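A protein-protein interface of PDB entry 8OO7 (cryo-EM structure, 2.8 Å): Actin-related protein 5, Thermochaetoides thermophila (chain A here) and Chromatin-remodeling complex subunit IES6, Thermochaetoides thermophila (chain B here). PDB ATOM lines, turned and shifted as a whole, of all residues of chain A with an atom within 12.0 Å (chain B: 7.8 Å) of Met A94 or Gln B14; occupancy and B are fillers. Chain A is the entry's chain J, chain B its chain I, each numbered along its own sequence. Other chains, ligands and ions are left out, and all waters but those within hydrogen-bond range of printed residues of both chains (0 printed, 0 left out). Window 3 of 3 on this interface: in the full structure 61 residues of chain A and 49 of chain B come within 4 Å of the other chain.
Among the printed residues, pairs that only touch across the chains: Tyr A106 with Leu B16, Tyr A38 with Gln B19, Tyr A38 with Leu B20, Asp A104 with Leu B20, Phe A35 with Leu B20, Phe A100 with Val B17, Phe A100 with Leu B20, Met A94 with Gln B14, Tyr A106 with Leu B20, Phe A98 with Glu B18 and Phe A35 with Leu B16.
Hydrophobic or aromatic side chains of chain B that line the printed part of chain A: Leu B16 and Leu B20. Among the printed residues, 12 pairs touch across the chains. Among the printed residues, Asp or Glu carboxylates within 4 Å of a Lys or Arg side-chain nitrogen of the other chain: Lys A96 with Glu B18.
Lys A93 touches none of the printed residues of chain B. Met A94 touches one residue of chain B. Of the printed residues of chain B, Lys A96 touches Glu B18 (2.9 Å). Printed residues of chain B within 4 Å of Phe A98: Glu B18. Printed residues of chain B within 4 Å of Tyr A106: Leu B16 and Leu B20. No residue of chain A comes within 4 Å of Gln B10. No residue of chain A comes within 4 Å of Ala B11. Gln B14 touches one residue of chain A. No residue of chain A comes within 4 Å of Ala B15. Leu B16 touches just these residues of chain A: Phe A35 and Tyr A106. Printed residues of chain A within 4 Å of Val B17: Phe A100 (3.7 Å). Printed residues of chain A within 4 Å of Gln B19: Tyr A38 (3.2 Å). The nearest residue of chain A that does not touch Gln B14 is Asp A91 (4.2 Å). The nearest printed residue of chain A that does not touch Gln B19 is Phe A100 (6.4 Å).
The side-chain carboxylate (OE1) of Glu B18 is in salt-bridge range of the side-chain amino group (NZ) of Lys A96, 2.9 Å away.
The backbone NH (N) of Phe A35 sits at hydrogen-bond distance from the backbone carbonyl oxygen (O) of Tyr A106 (2.9 Å). O of Phe A98 lies within hydrogen-bond range of N of Tyr A89. The backbone carbonyl oxygen of Lys A96 sits at hydrogen-bond distance from the backbone NH of Asp A91 (3.2 Å).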
ATOM      1  N   PHE A  35     -11.245 -25.137 -16.396  1.00  0.00           N
ATOM      2  CA  PHE A  35     -10.221 -26.113 -16.042  1.00  0.00           C
ATOM      3  C   PHE A  35     -10.612 -26.874 -14.782  1.00  0.00           C
ATOM      4  O   PHE A  35     -11.170 -26.302 -13.842  1.00  0.00           O
ATOM      5  CB  PHE A  35      -8.877 -25.409 -15.846  1.00  0.00           C
ATOM      6  CG  PHE A  35      -7.810 -26.281 -15.251  1.00  0.00           C
ATOM      7  CD1 PHE A  35      -7.078 -27.143 -16.047  1.00  0.00           C
ATOM      8  CD2 PHE A  35      -7.525 -26.220 -13.897  1.00  0.00           C
ATOM      9  CE1 PHE A  35      -6.096 -27.941 -15.502  1.00  0.00           C
ATOM     10  CE2 PHE A  35      -6.543 -27.013 -13.348  1.00  0.00           C
ATOM     11  CZ  PHE A  35      -5.827 -27.875 -14.152  1.00  0.00           C
ATOM     12  N   TYR A  38      -5.213 -31.553 -13.683  1.00  0.00           N
ATOM     13  CA  TYR A  38      -4.126 -32.016 -14.539  1.00  0.00           C
ATOM     14  C   TYR A  38      -4.368 -33.450 -14.995  1.00  0.00           C
ATOM     15  O   TYR A  38      -4.728 -34.317 -14.193  1.00  0.00           O
ATOM     16  CB  TYR A  38      -2.784 -31.916 -13.816  1.00  0.00           C
ATOM     17  CG  TYR A  38      -1.612 -32.286 -14.698  1.00  0.00           C
ATOM     18  CD1 TYR A  38      -1.347 -31.579 -15.861  1.00  0.00           C
ATOM     19  CD2 TYR A  38      -0.773 -33.340 -14.370  1.00  0.00           C
ATOM     20  CE1 TYR A  38      -0.293 -31.920 -16.681  1.00  0.00           C
ATOM     21  CE2 TYR A  38       0.297 -33.678 -15.178  1.00  0.00           C
ATOM     22  CZ  TYR A  38       0.528 -32.967 -16.334  1.00  0.00           C
ATOM     23  OH  TYR A  38       1.596 -33.292 -17.136  1.00  0.00           O
ATOM     24  N   TYR A  89       0.881 -17.263 -25.086  1.00  0.00           N
ATOM     25  CA  TYR A  89       1.195 -15.875 -24.771  1.00  0.00           C
ATOM     26  C   TYR A  89       2.563 -15.761 -24.106  1.00  0.00           C
ATOM     27  O   TYR A  89       3.064 -16.705 -23.490  1.00  0.00           O
ATOM     28  CB  TYR A  89       0.118 -15.264 -23.865  1.00  0.00           C
ATOM     29  CG  TYR A  89       0.016 -15.916 -22.502  1.00  0.00           C
ATOM     30  CD1 TYR A  89      -0.827 -16.995 -22.291  1.00  0.00           C
ATOM     31  CD2 TYR A  89       0.751 -15.443 -21.424  1.00  0.00           C
ATOM     32  CE1 TYR A  89      -0.922 -17.598 -21.053  1.00  0.00           C
ATOM     33  CE2 TYR A  89       0.657 -16.036 -20.179  1.00  0.00           C
ATOM     34  CZ  TYR A  89      -0.180 -17.113 -20.001  1.00  0.00           C
ATOM     35  OH  TYR A  89      -0.285 -17.703 -18.763  1.00  0.00           O
ATOM     36  N   ARG A  90       3.154 -14.572 -24.242  1.00  0.00           N
ATOM     37  CA  ARG A  90       4.370 -14.184 -23.530  1.00  0.00           C
ATOM     38  C   ARG A  90       4.030 -13.667 -22.135  1.00  0.00           C
ATOM     39  O   ARG A  90       3.285 -12.690 -22.000  1.00  0.00           O
ATOM     40  CB  ARG A  90       5.122 -13.115 -24.316  1.00  0.00           C
ATOM     41  CG  ARG A  90       5.560 -13.545 -25.699  1.00  0.00           C
ATOM     42  CD  ARG A  90       5.925 -12.333 -26.534  1.00  0.00           C
ATOM     43  NE  ARG A  90       4.753 -11.516 -26.829  1.00  0.00           N
ATOM     44  CZ  ARG A  90       4.577 -10.829 -27.949  1.00  0.00           C
ATOM     45  NH1 ARG A  90       5.500 -10.801 -28.896  1.00  0.00           N
ATOM     46  NH2 ARG A  90       3.450 -10.142 -28.117  1.00  0.00           N
ATOM     47  N   ASP A  91       4.577 -14.300 -21.100  1.00  0.00           N
ATOM     48  CA  ASP A  91       4.435 -13.780 -19.739  1.00  0.00           C
ATOM     49  C   ASP A  91       5.467 -12.676 -19.515  1.00  0.00           C
ATOM     50  O   ASP A  91       6.566 -12.915 -19.012  1.00  0.00           O
ATOM     51  CB  ASP A  91       4.595 -14.899 -18.718  1.00  0.00           C
ATOM     52  CG  ASP A  91       4.280 -14.450 -17.308  1.00  0.00           C
ATOM     53  OD1 ASP A  91       3.700 -13.357 -17.148  1.00  0.00           O
ATOM     54  OD2 ASP A  91       4.618 -15.186 -16.357  1.00  0.00           O
ATOM     55  N   ARG A  92       5.097 -11.450 -19.906  1.00  0.00           N
ATOM     56  CA  ARG A  92       6.070 -10.375 -20.111  1.00  0.00           C
ATOM     57  C   ARG A  92       6.961 -10.141 -18.895  1.00  0.00           C
ATOM     58  O   ARG A  92       8.152  -9.841 -19.038  1.00  0.00           O
ATOM     59  CB  ARG A  92       5.363  -9.070 -20.488  1.00  0.00           C
ATOM     60  CG  ARG A  92       4.452  -9.150 -21.698  1.00  0.00           C
ATOM     61  CD  ARG A  92       4.177  -7.753 -22.240  1.00  0.00           C
ATOM     62  NE  ARG A  92       3.673  -6.849 -21.212  1.00  0.00           N
ATOM     63  CZ  ARG A  92       2.931  -5.776 -21.453  1.00  0.00           C
ATOM     64  NH1 ARG A  92       2.506  -5.488 -22.672  1.00  0.00           N
ATOM     65  NH2 ARG A  92       2.588  -4.984 -20.440  1.00  0.00           N
ATOM     66  N   LYS A  93       6.405 -10.275 -17.689  1.00  0.00           N
ATOM     67  CA  LYS A  93       7.182 -10.080 -16.468  1.00  0.00           C
ATOM     68  C   LYS A  93       8.145 -11.222 -16.171  1.00  0.00           C
ATOM     69  O   LYS A  93       9.027 -11.051 -15.321  1.00  0.00           O
ATOM     70  CB  LYS A  93       6.248  -9.867 -15.275  1.00  0.00           C
ATOM     71  CG  LYS A  93       5.416 -11.075 -14.890  1.00  0.00           C
ATOM     72  CD  LYS A  93       4.555 -10.768 -13.675  1.00  0.00           C
ATOM     73  CE  LYS A  93       3.711 -11.965 -13.270  1.00  0.00           C
ATOM     74  NZ  LYS A  93       2.887 -11.674 -12.066  1.00  0.00           N
ATOM     75  N   MET A  94       8.011 -12.368 -16.834  1.00  0.00           N
ATOM     76  CA  MET A  94       8.853 -13.518 -16.551  1.00  0.00           C
ATOM     77  C   MET A  94       9.621 -13.994 -17.775  1.00  0.00           C
ATOM     78  O   MET A  94      10.529 -14.821 -17.636  1.00  0.00           O
ATOM     79  CB  MET A  94       8.007 -14.673 -15.987  1.00  0.00           C
ATOM     80  CG  MET A  94       8.795 -15.740 -15.244  1.00  0.00           C
ATOM     81  SD  MET A  94       7.734 -16.857 -14.307  1.00  0.00           S
ATOM     82  CE  MET A  94       8.951 -17.954 -13.584  1.00  0.00           C
ATOM     83  N   GLY A  95       9.295 -13.483 -18.958  1.00  0.00           N
ATOM     84  CA  GLY A  95      10.078 -13.689 -20.159  1.00  0.00           C
ATOM     85  C   GLY A  95       9.857 -15.011 -20.861  1.00  0.00           C
ATOM     86  O   GLY A  95       9.982 -15.087 -22.087  1.00  0.00           O
ATOM     87  N   LYS A  96       9.526 -16.058 -20.109  1.00  0.00           N
ATOM     88  CA  LYS A  96       9.183 -17.329 -20.730  1.00  0.00           C
ATOM     89  C   LYS A  96       7.845 -17.222 -21.450  1.00  0.00           C
ATOM     90  O   LYS A  96       6.922 -16.546 -20.988  1.00  0.00           O
ATOM     91  CB  LYS A  96       9.169 -18.448 -19.688  1.00  0.00           C
ATOM     92  CG  LYS A  96       8.328 -18.180 -18.458  1.00  0.00           C
ATOM     93  CD  LYS A  96       8.184 -19.451 -17.639  1.00  0.00           C
ATOM     94  CE  LYS A  96       9.542 -20.054 -17.312  1.00  0.00           C
ATOM     95  NZ  LYS A  96       9.430 -21.243 -16.422  1.00  0.00           N
ATOM     96  N   THR A  97       7.745 -17.901 -22.587  1.00  0.00           N
ATOM     97  CA  THR A  97       6.469 -18.126 -23.247  1.00  0.00           C
ATOM     98  C   THR A  97       5.740 -19.309 -22.616  1.00  0.00           C
ATOM     99  O   THR A  97       6.356 -20.286 -22.180  1.00  0.00           O
ATOM    100  CB  THR A  97       6.692 -18.363 -24.745  1.00  0.00           C
ATOM    101  OG1 THR A  97       7.236 -17.178 -25.338  1.00  0.00           O
ATOM    102  CG2 THR A  97       5.391 -18.700 -25.453  1.00  0.00           C
ATOM    103  N   PHE A  98       4.412 -19.211 -22.572  1.00  0.00           N
ATOM    104  CA  PHE A  98       3.547 -20.343 -22.286  1.00  0.00           C
ATOM    105  C   PHE A  98       2.667 -20.615 -23.496  1.00  0.00           C
ATOM    106  O   PHE A  98       2.318 -19.698 -24.245  1.00  0.00           O
ATOM    107  CB  PHE A  98       2.654 -20.081 -21.068  1.00  0.00           C
ATOM    108  CG  PHE A  98       3.403 -19.909 -19.783  1.00  0.00           C
ATOM    109  CD1 PHE A  98       4.169 -20.940 -19.272  1.00  0.00           C
ATOM    110  CD2 PHE A  98       3.326 -18.721 -19.078  1.00  0.00           C
ATOM    111  CE1 PHE A  98       4.851 -20.787 -18.085  1.00  0.00           C
ATOM    112  CE2 PHE A  98       4.005 -18.561 -17.891  1.00  0.00           C
ATOM    113  CZ  PHE A  98       4.768 -19.595 -17.393  1.00  0.00           C
ATOM    114  N   SER A  99       2.321 -21.886 -23.689  1.00  0.00           N
ATOM    115  CA  SER A  99       1.232 -22.252 -24.581  1.00  0.00           C
ATOM    116  C   SER A  99       0.405 -23.363 -23.960  1.00  0.00           C
ATOM    117  O   SER A  99       0.931 -24.240 -23.270  1.00  0.00           O
ATOM    118  CB  SER A  99       1.753 -22.700 -25.952  1.00  0.00           C
ATOM    119  OG  SER A  99       2.316 -23.999 -25.884  1.00  0.00           O
ATOM    120  N   PHE A 100      -0.898 -23.302 -24.206  1.00  0.00           N
ATOM    121  CA  PHE A 100      -1.876 -24.250 -23.700  1.00  0.00           C
ATOM    122  C   PHE A 100      -2.728 -24.689 -24.880  1.00  0.00           C
ATOM    123  O   PHE A 100      -2.821 -23.980 -25.882  1.00  0.00           O
ATOM    124  CB  PHE A 100      -2.724 -23.636 -22.585  1.00  0.00           C
ATOM    125  CG  PHE A 100      -1.910 -23.049 -21.469  1.00  0.00           C
ATOM    126  CD1 PHE A 100      -1.310 -23.865 -20.527  1.00  0.00           C
ATOM    127  CD2 PHE A 100      -1.730 -21.679 -21.374  1.00  0.00           C
ATOM    128  CE1 PHE A 100      -0.555 -23.325 -19.505  1.00  0.00           C
ATOM    129  CE2 PHE A 100      -0.977 -21.134 -20.357  1.00  0.00           C
ATOM    130  CZ  PHE A 100      -0.387 -21.960 -19.420  1.00  0.00           C
ATOM    131  N   ASP A 104      -6.498 -26.987 -20.555  1.00  0.00           N
ATOM    132  CA  ASP A 104      -5.445 -26.246 -19.882  1.00  0.00           C
ATOM    133  C   ASP A 104      -5.457 -24.773 -20.254  1.00  0.00           C
ATOM    134  O   ASP A 104      -4.967 -23.951 -19.473  1.00  0.00           O
ATOM    135  CB  ASP A 104      -4.081 -26.863 -20.202  1.00  0.00           C
ATOM    136  CG  ASP A 104      -3.787 -26.892 -21.690  1.00  0.00           C
ATOM    137  OD1 ASP A 104      -4.745 -26.830 -22.487  1.00  0.00           O
ATOM    138  OD2 ASP A 104      -2.597 -26.981 -22.064  1.00  0.00           O
ATOM    139  N   TYR A 106      -7.890 -22.116 -19.694  1.00  0.00           N
ATOM    140  CA  TYR A 106      -8.752 -22.299 -18.530  1.00  0.00           C
ATOM    141  C   TYR A 106     -10.237 -22.369 -18.865  1.00  0.00           C
ATOM    142  O   TYR A 106     -11.033 -22.690 -17.975  1.00  0.00           O
ATOM    143  CB  TYR A 106      -8.470 -21.220 -17.488  1.00  0.00           C
ATOM    144  CG  TYR A 106      -7.401 -21.677 -16.524  1.00  0.00           C
ATOM    145  CD1 TYR A 106      -6.115 -21.944 -16.971  1.00  0.00           C
ATOM    146  CD2 TYR A 106      -7.685 -21.889 -15.184  1.00  0.00           C
ATOM    147  CE1 TYR A 106      -5.133 -22.368 -16.107  1.00  0.00           C
ATOM    148  CE2 TYR A 106      -6.707 -22.325 -14.312  1.00  0.00           C
ATOM    149  CZ  TYR A 106      -5.433 -22.560 -14.781  1.00  0.00           C
ATOM    150  OH  TYR A 106      -4.452 -23.004 -13.927  1.00  0.00           O
ATOM    151  N   ALA A 111      -5.665 -18.437 -17.414  1.00  0.00           N
ATOM    152  CA  ALA A 111      -6.547 -17.456 -16.790  1.00  0.00           C
ATOM    153  C   ALA A 111      -6.447 -16.102 -17.489  1.00  0.00           C
ATOM    154  O   ALA A 111      -7.215 -15.184 -17.202  1.00  0.00           O
ATOM    155  CB  ALA A 111      -6.221 -17.316 -15.312  1.00  0.00           C
ATOM    156  N   ARG A 112      -5.489 -15.987 -18.410  1.00  0.00           N
ATOM    157  CA  ARG A 112      -5.480 -14.870 -19.348  1.00  0.00           C
ATOM    158  C   ARG A 112      -6.402 -15.121 -20.535  1.00  0.00           C
ATOM    159  O   ARG A 112      -6.948 -14.167 -21.103  1.00  0.00           O
ATOM    160  CB  ARG A 112      -4.053 -14.598 -19.822  1.00  0.00           C
ATOM    161  CG  ARG A 112      -3.182 -13.954 -18.754  1.00  0.00           C
ATOM    162  CD  ARG A 112      -1.882 -13.413 -19.324  1.00  0.00           C
ATOM    163  NE  ARG A 112      -1.340 -12.333 -18.508  1.00  0.00           N
ATOM    164  CZ  ARG A 112      -1.843 -11.107 -18.447  1.00  0.00           C
ATOM    165  NH1 ARG A 112      -2.875 -10.744 -19.190  1.00  0.00           N
ATOM    166  NH2 ARG A 112      -1.285 -10.217 -17.630  1.00  0.00           N
ATOM    167  N   GLN B   7       3.501 -15.285  -1.797  1.00  0.00           N
ATOM    168  CA  GLN B   7       2.328 -15.898  -1.186  1.00  0.00           C
ATOM    169  C   GLN B   7       1.983 -17.211  -1.885  1.00  0.00           C
ATOM    170  O   GLN B   7       2.118 -17.331  -3.103  1.00  0.00           O
ATOM    171  CB  GLN B   7       1.135 -14.938  -1.216  1.00  0.00           C
ATOM    172  CG  GLN B   7      -0.104 -15.465  -0.507  1.00  0.00           C
ATOM    173  CD  GLN B   7      -1.169 -14.403  -0.320  1.00  0.00           C
ATOM    174  OE1 GLN B   7      -1.035 -13.281  -0.807  1.00  0.00           O
ATOM    175  NE2 GLN B   7      -2.234 -14.753   0.393  1.00  0.00           N
ATOM    176  N   SER B   8       1.548 -18.191  -1.088  1.00  0.00           N
ATOM    177  CA  SER B   8       1.385 -19.558  -1.576  1.00  0.00           C
ATOM    178  C   SER B   8       0.434 -19.631  -2.766  1.00  0.00           C
ATOM    179  O   SER B   8       0.630 -20.448  -3.674  1.00  0.00           O
ATOM    180  CB  SER B   8       0.891 -20.459  -0.444  1.00  0.00           C
ATOM    181  OG  SER B   8       1.734 -20.359   0.690  1.00  0.00           O
ATOM    182  N   ALA B   9      -0.603 -18.790  -2.780  1.00  0.00           N
ATOM    183  CA  ALA B   9      -1.536 -18.786  -3.904  1.00  0.00           C
ATOM    184  C   ALA B   9      -0.846 -18.413  -5.212  1.00  0.00           C
ATOM    185  O   ALA B   9      -1.106 -19.027  -6.253  1.00  0.00           O
ATOM    186  CB  ALA B   9      -2.692 -17.828  -3.619  1.00  0.00           C
ATOM    187  N   GLN B  10       0.033 -17.410  -5.183  1.00  0.00           N
ATOM    188  CA  GLN B  10       0.802 -17.074  -6.379  1.00  0.00           C
ATOM    189  C   GLN B  10       1.788 -18.180  -6.742  1.00  0.00           C
ATOM    190  O   GLN B  10       1.947 -18.513  -7.923  1.00  0.00           O
ATOM    191  CB  GLN B  10       1.539 -15.750  -6.174  1.00  0.00           C
ATOM    192  CG  GLN B  10       0.642 -14.520  -6.142  1.00  0.00           C
ATOM    193  CD  GLN B  10       0.077 -14.154  -7.506  1.00  0.00           C
ATOM    194  OE1 GLN B  10       0.374 -14.798  -8.512  1.00  0.00           O
ATOM    195  NE2 GLN B  10      -0.740 -13.109  -7.542  1.00  0.00           N
ATOM    196  N   ALA B  11       2.466 -18.748  -5.745  1.00  0.00           N
ATOM    197  CA  ALA B  11       3.386 -19.857  -5.988  1.00  0.00           C
ATOM    198  C   ALA B  11       2.667 -21.082  -6.544  1.00  0.00           C
ATOM    199  O   ALA B  11       3.137 -21.710  -7.501  1.00  0.00           O
ATOM    200  CB  ALA B  11       4.126 -20.210  -4.697  1.00  0.00           C
ATOM    201  N   ALA B  12       1.525 -21.440  -5.954  1.00  0.00           N
ATOM    202  CA  ALA B  12       0.748 -22.572  -6.452  1.00  0.00           C
ATOM    203  C   ALA B  12       0.263 -22.358  -7.883  1.00  0.00           C
ATOM    204  O   ALA B  12       0.341 -23.271  -8.713  1.00  0.00           O
ATOM    205  CB  ALA B  12      -0.438 -22.839  -5.527  1.00  0.00           C
ATOM    206  N   HIS B  13      -0.241 -21.164  -8.191  1.00  0.00           N
ATOM    207  CA  HIS B  13      -0.658 -20.865  -9.559  1.00  0.00           C
ATOM    208  C   HIS B  13       0.511 -20.904 -10.538  1.00  0.00           C
ATOM    209  O   HIS B  13       0.374 -21.416 -11.656  1.00  0.00           O
ATOM    210  CB  HIS B  13      -1.351 -19.504  -9.605  1.00  0.00           C
ATOM    211  CG  HIS B  13      -2.026 -19.214 -10.909  1.00  0.00           C
ATOM    212  ND1 HIS B  13      -1.413 -18.522 -11.930  1.00  0.00           N
ATOM    213  CD2 HIS B  13      -3.265 -19.526 -11.357  1.00  0.00           C
ATOM    214  CE1 HIS B  13      -2.244 -18.420 -12.950  1.00  0.00           C
ATOM    215  NE2 HIS B  13      -3.375 -19.020 -12.629  1.00  0.00           N
ATOM    216  N   GLN B  14       1.665 -20.363 -10.144  1.00  0.00           N
ATOM    217  CA  GLN B  14       2.862 -20.464 -10.976  1.00  0.00           C
ATOM    218  C   GLN B  14       3.303 -21.910 -11.184  1.00  0.00           C
ATOM    219  O   GLN B  14       3.749 -22.278 -12.277  1.00  0.00           O
ATOM    220  CB  GLN B  14       3.999 -19.643 -10.368  1.00  0.00           C
ATOM    221  CG  GLN B  14       3.914 -18.157 -10.667  1.00  0.00           C
ATOM    222  CD  GLN B  14       4.136 -17.837 -12.135  1.00  0.00           C
ATOM    223  OE1 GLN B  14       4.614 -18.673 -12.902  1.00  0.00           O
ATOM    224  NE2 GLN B  14       3.788 -16.618 -12.532  1.00  0.00           N
ATOM    225  N   ALA B  15       3.216 -22.736 -10.143  1.00  0.00           N
ATOM    226  CA  ALA B  15       3.483 -24.162 -10.308  1.00  0.00           C
ATOM    227  C   ALA B  15       2.518 -24.805 -11.300  1.00  0.00           C
ATOM    228  O   ALA B  15       2.932 -25.569 -12.179  1.00  0.00           O
ATOM    229  CB  ALA B  15       3.406 -24.867  -8.953  1.00  0.00           C
ATOM    230  N   LEU B  16       1.227 -24.502 -11.176  1.00  0.00           N
ATOM    231  CA  LEU B  16       0.219 -25.111 -12.038  1.00  0.00           C
ATOM    232  C   LEU B  16       0.341 -24.684 -13.500  1.00  0.00           C
ATOM    233  O   LEU B  16       0.183 -25.517 -14.400  1.00  0.00           O
ATOM    234  CB  LEU B  16      -1.176 -24.788 -11.504  1.00  0.00           C
ATOM    235  CG  LEU B  16      -2.365 -25.440 -12.211  1.00  0.00           C
ATOM    236  CD1 LEU B  16      -2.242 -26.953 -12.187  1.00  0.00           C
ATOM    237  CD2 LEU B  16      -3.661 -25.008 -11.553  1.00  0.00           C
ATOM    238  N   VAL B  17       0.622 -23.406 -13.769  1.00  0.00           N
ATOM    239  CA  VAL B  17       0.829 -22.998 -15.160  1.00  0.00           C
ATOM    240  C   VAL B  17       2.094 -23.603 -15.766  1.00  0.00           C
ATOM    241  O   VAL B  17       2.129 -23.892 -16.969  1.00  0.00           O
ATOM    242  CB  VAL B  17       0.837 -21.460 -15.280  1.00  0.00           C
ATOM    243  CG1 VAL B  17      -0.521 -20.886 -14.899  1.00  0.00           C
ATOM    244  CG2 VAL B  17       1.940 -20.851 -14.436  1.00  0.00           C
ATOM    245  N   GLU B  18       3.151 -23.797 -14.977  1.00  0.00           N
ATOM    246  CA  GLU B  18       4.314 -24.513 -15.492  1.00  0.00           C
ATOM    247  C   GLU B  18       4.011 -25.995 -15.696  1.00  0.00           C
ATOM    248  O   GLU B  18       4.449 -26.597 -16.683  1.00  0.00           O
ATOM    249  CB  GLU B  18       5.508 -24.326 -14.556  1.00  0.00           C
ATOM    250  CG  GLU B  18       6.775 -25.040 -15.010  1.00  0.00           C
ATOM    251  CD  GLU B  18       7.291 -24.521 -16.339  1.00  0.00           C
ATOM    252  OE1 GLU B  18       7.383 -23.286 -16.500  1.00  0.00           O
ATOM    253  OE2 GLU B  18       7.615 -25.347 -17.219  1.00  0.00           O
ATOM    254  N   GLN B  19       3.255 -26.590 -14.772  1.00  0.00           N
ATOM    255  CA  GLN B  19       2.834 -27.982 -14.908  1.00  0.00           C
ATOM    256  C   GLN B  19       1.974 -28.204 -16.149  1.00  0.00           C
ATOM    257  O   GLN B  19       2.086 -29.241 -16.813  1.00  0.00           O
ATOM    258  CB  GLN B  19       2.084 -28.410 -13.645  1.00  0.00           C
ATOM    259  CG  GLN B  19       1.545 -29.823 -13.665  1.00  0.00           C
ATOM    260  CD  GLN B  19       1.043 -30.259 -12.304  1.00  0.00           C
ATOM    261  OE1 GLN B  19       0.898 -29.443 -11.394  1.00  0.00           O
ATOM    262  NE2 GLN B  19       0.784 -31.552 -12.153  1.00  0.00           N
ATOM    263  N   LEU B  20       1.110 -27.245 -16.476  1.00  0.00           N
ATOM    264  CA  LEU B  20       0.224 -27.369 -17.630  1.00  0.00           C
ATOM    265  C   LEU B  20       0.883 -26.990 -18.952  1.00  0.00           C
ATOM    266  O   LEU B  20       0.427 -27.445 -20.006  1.00  0.00           O
ATOM    267  CB  LEU B  20      -1.026 -26.518 -17.415  1.00  0.00           C
ATOM    268  CG  LEU B  20      -1.956 -27.006 -16.303  1.00  0.00           C
ATOM    269  CD1 LEU B  20      -2.993 -25.948 -15.982  1.00  0.00           C
ATOM    270  CD2 LEU B  20      -2.619 -28.310 -16.692  1.00  0.00           C
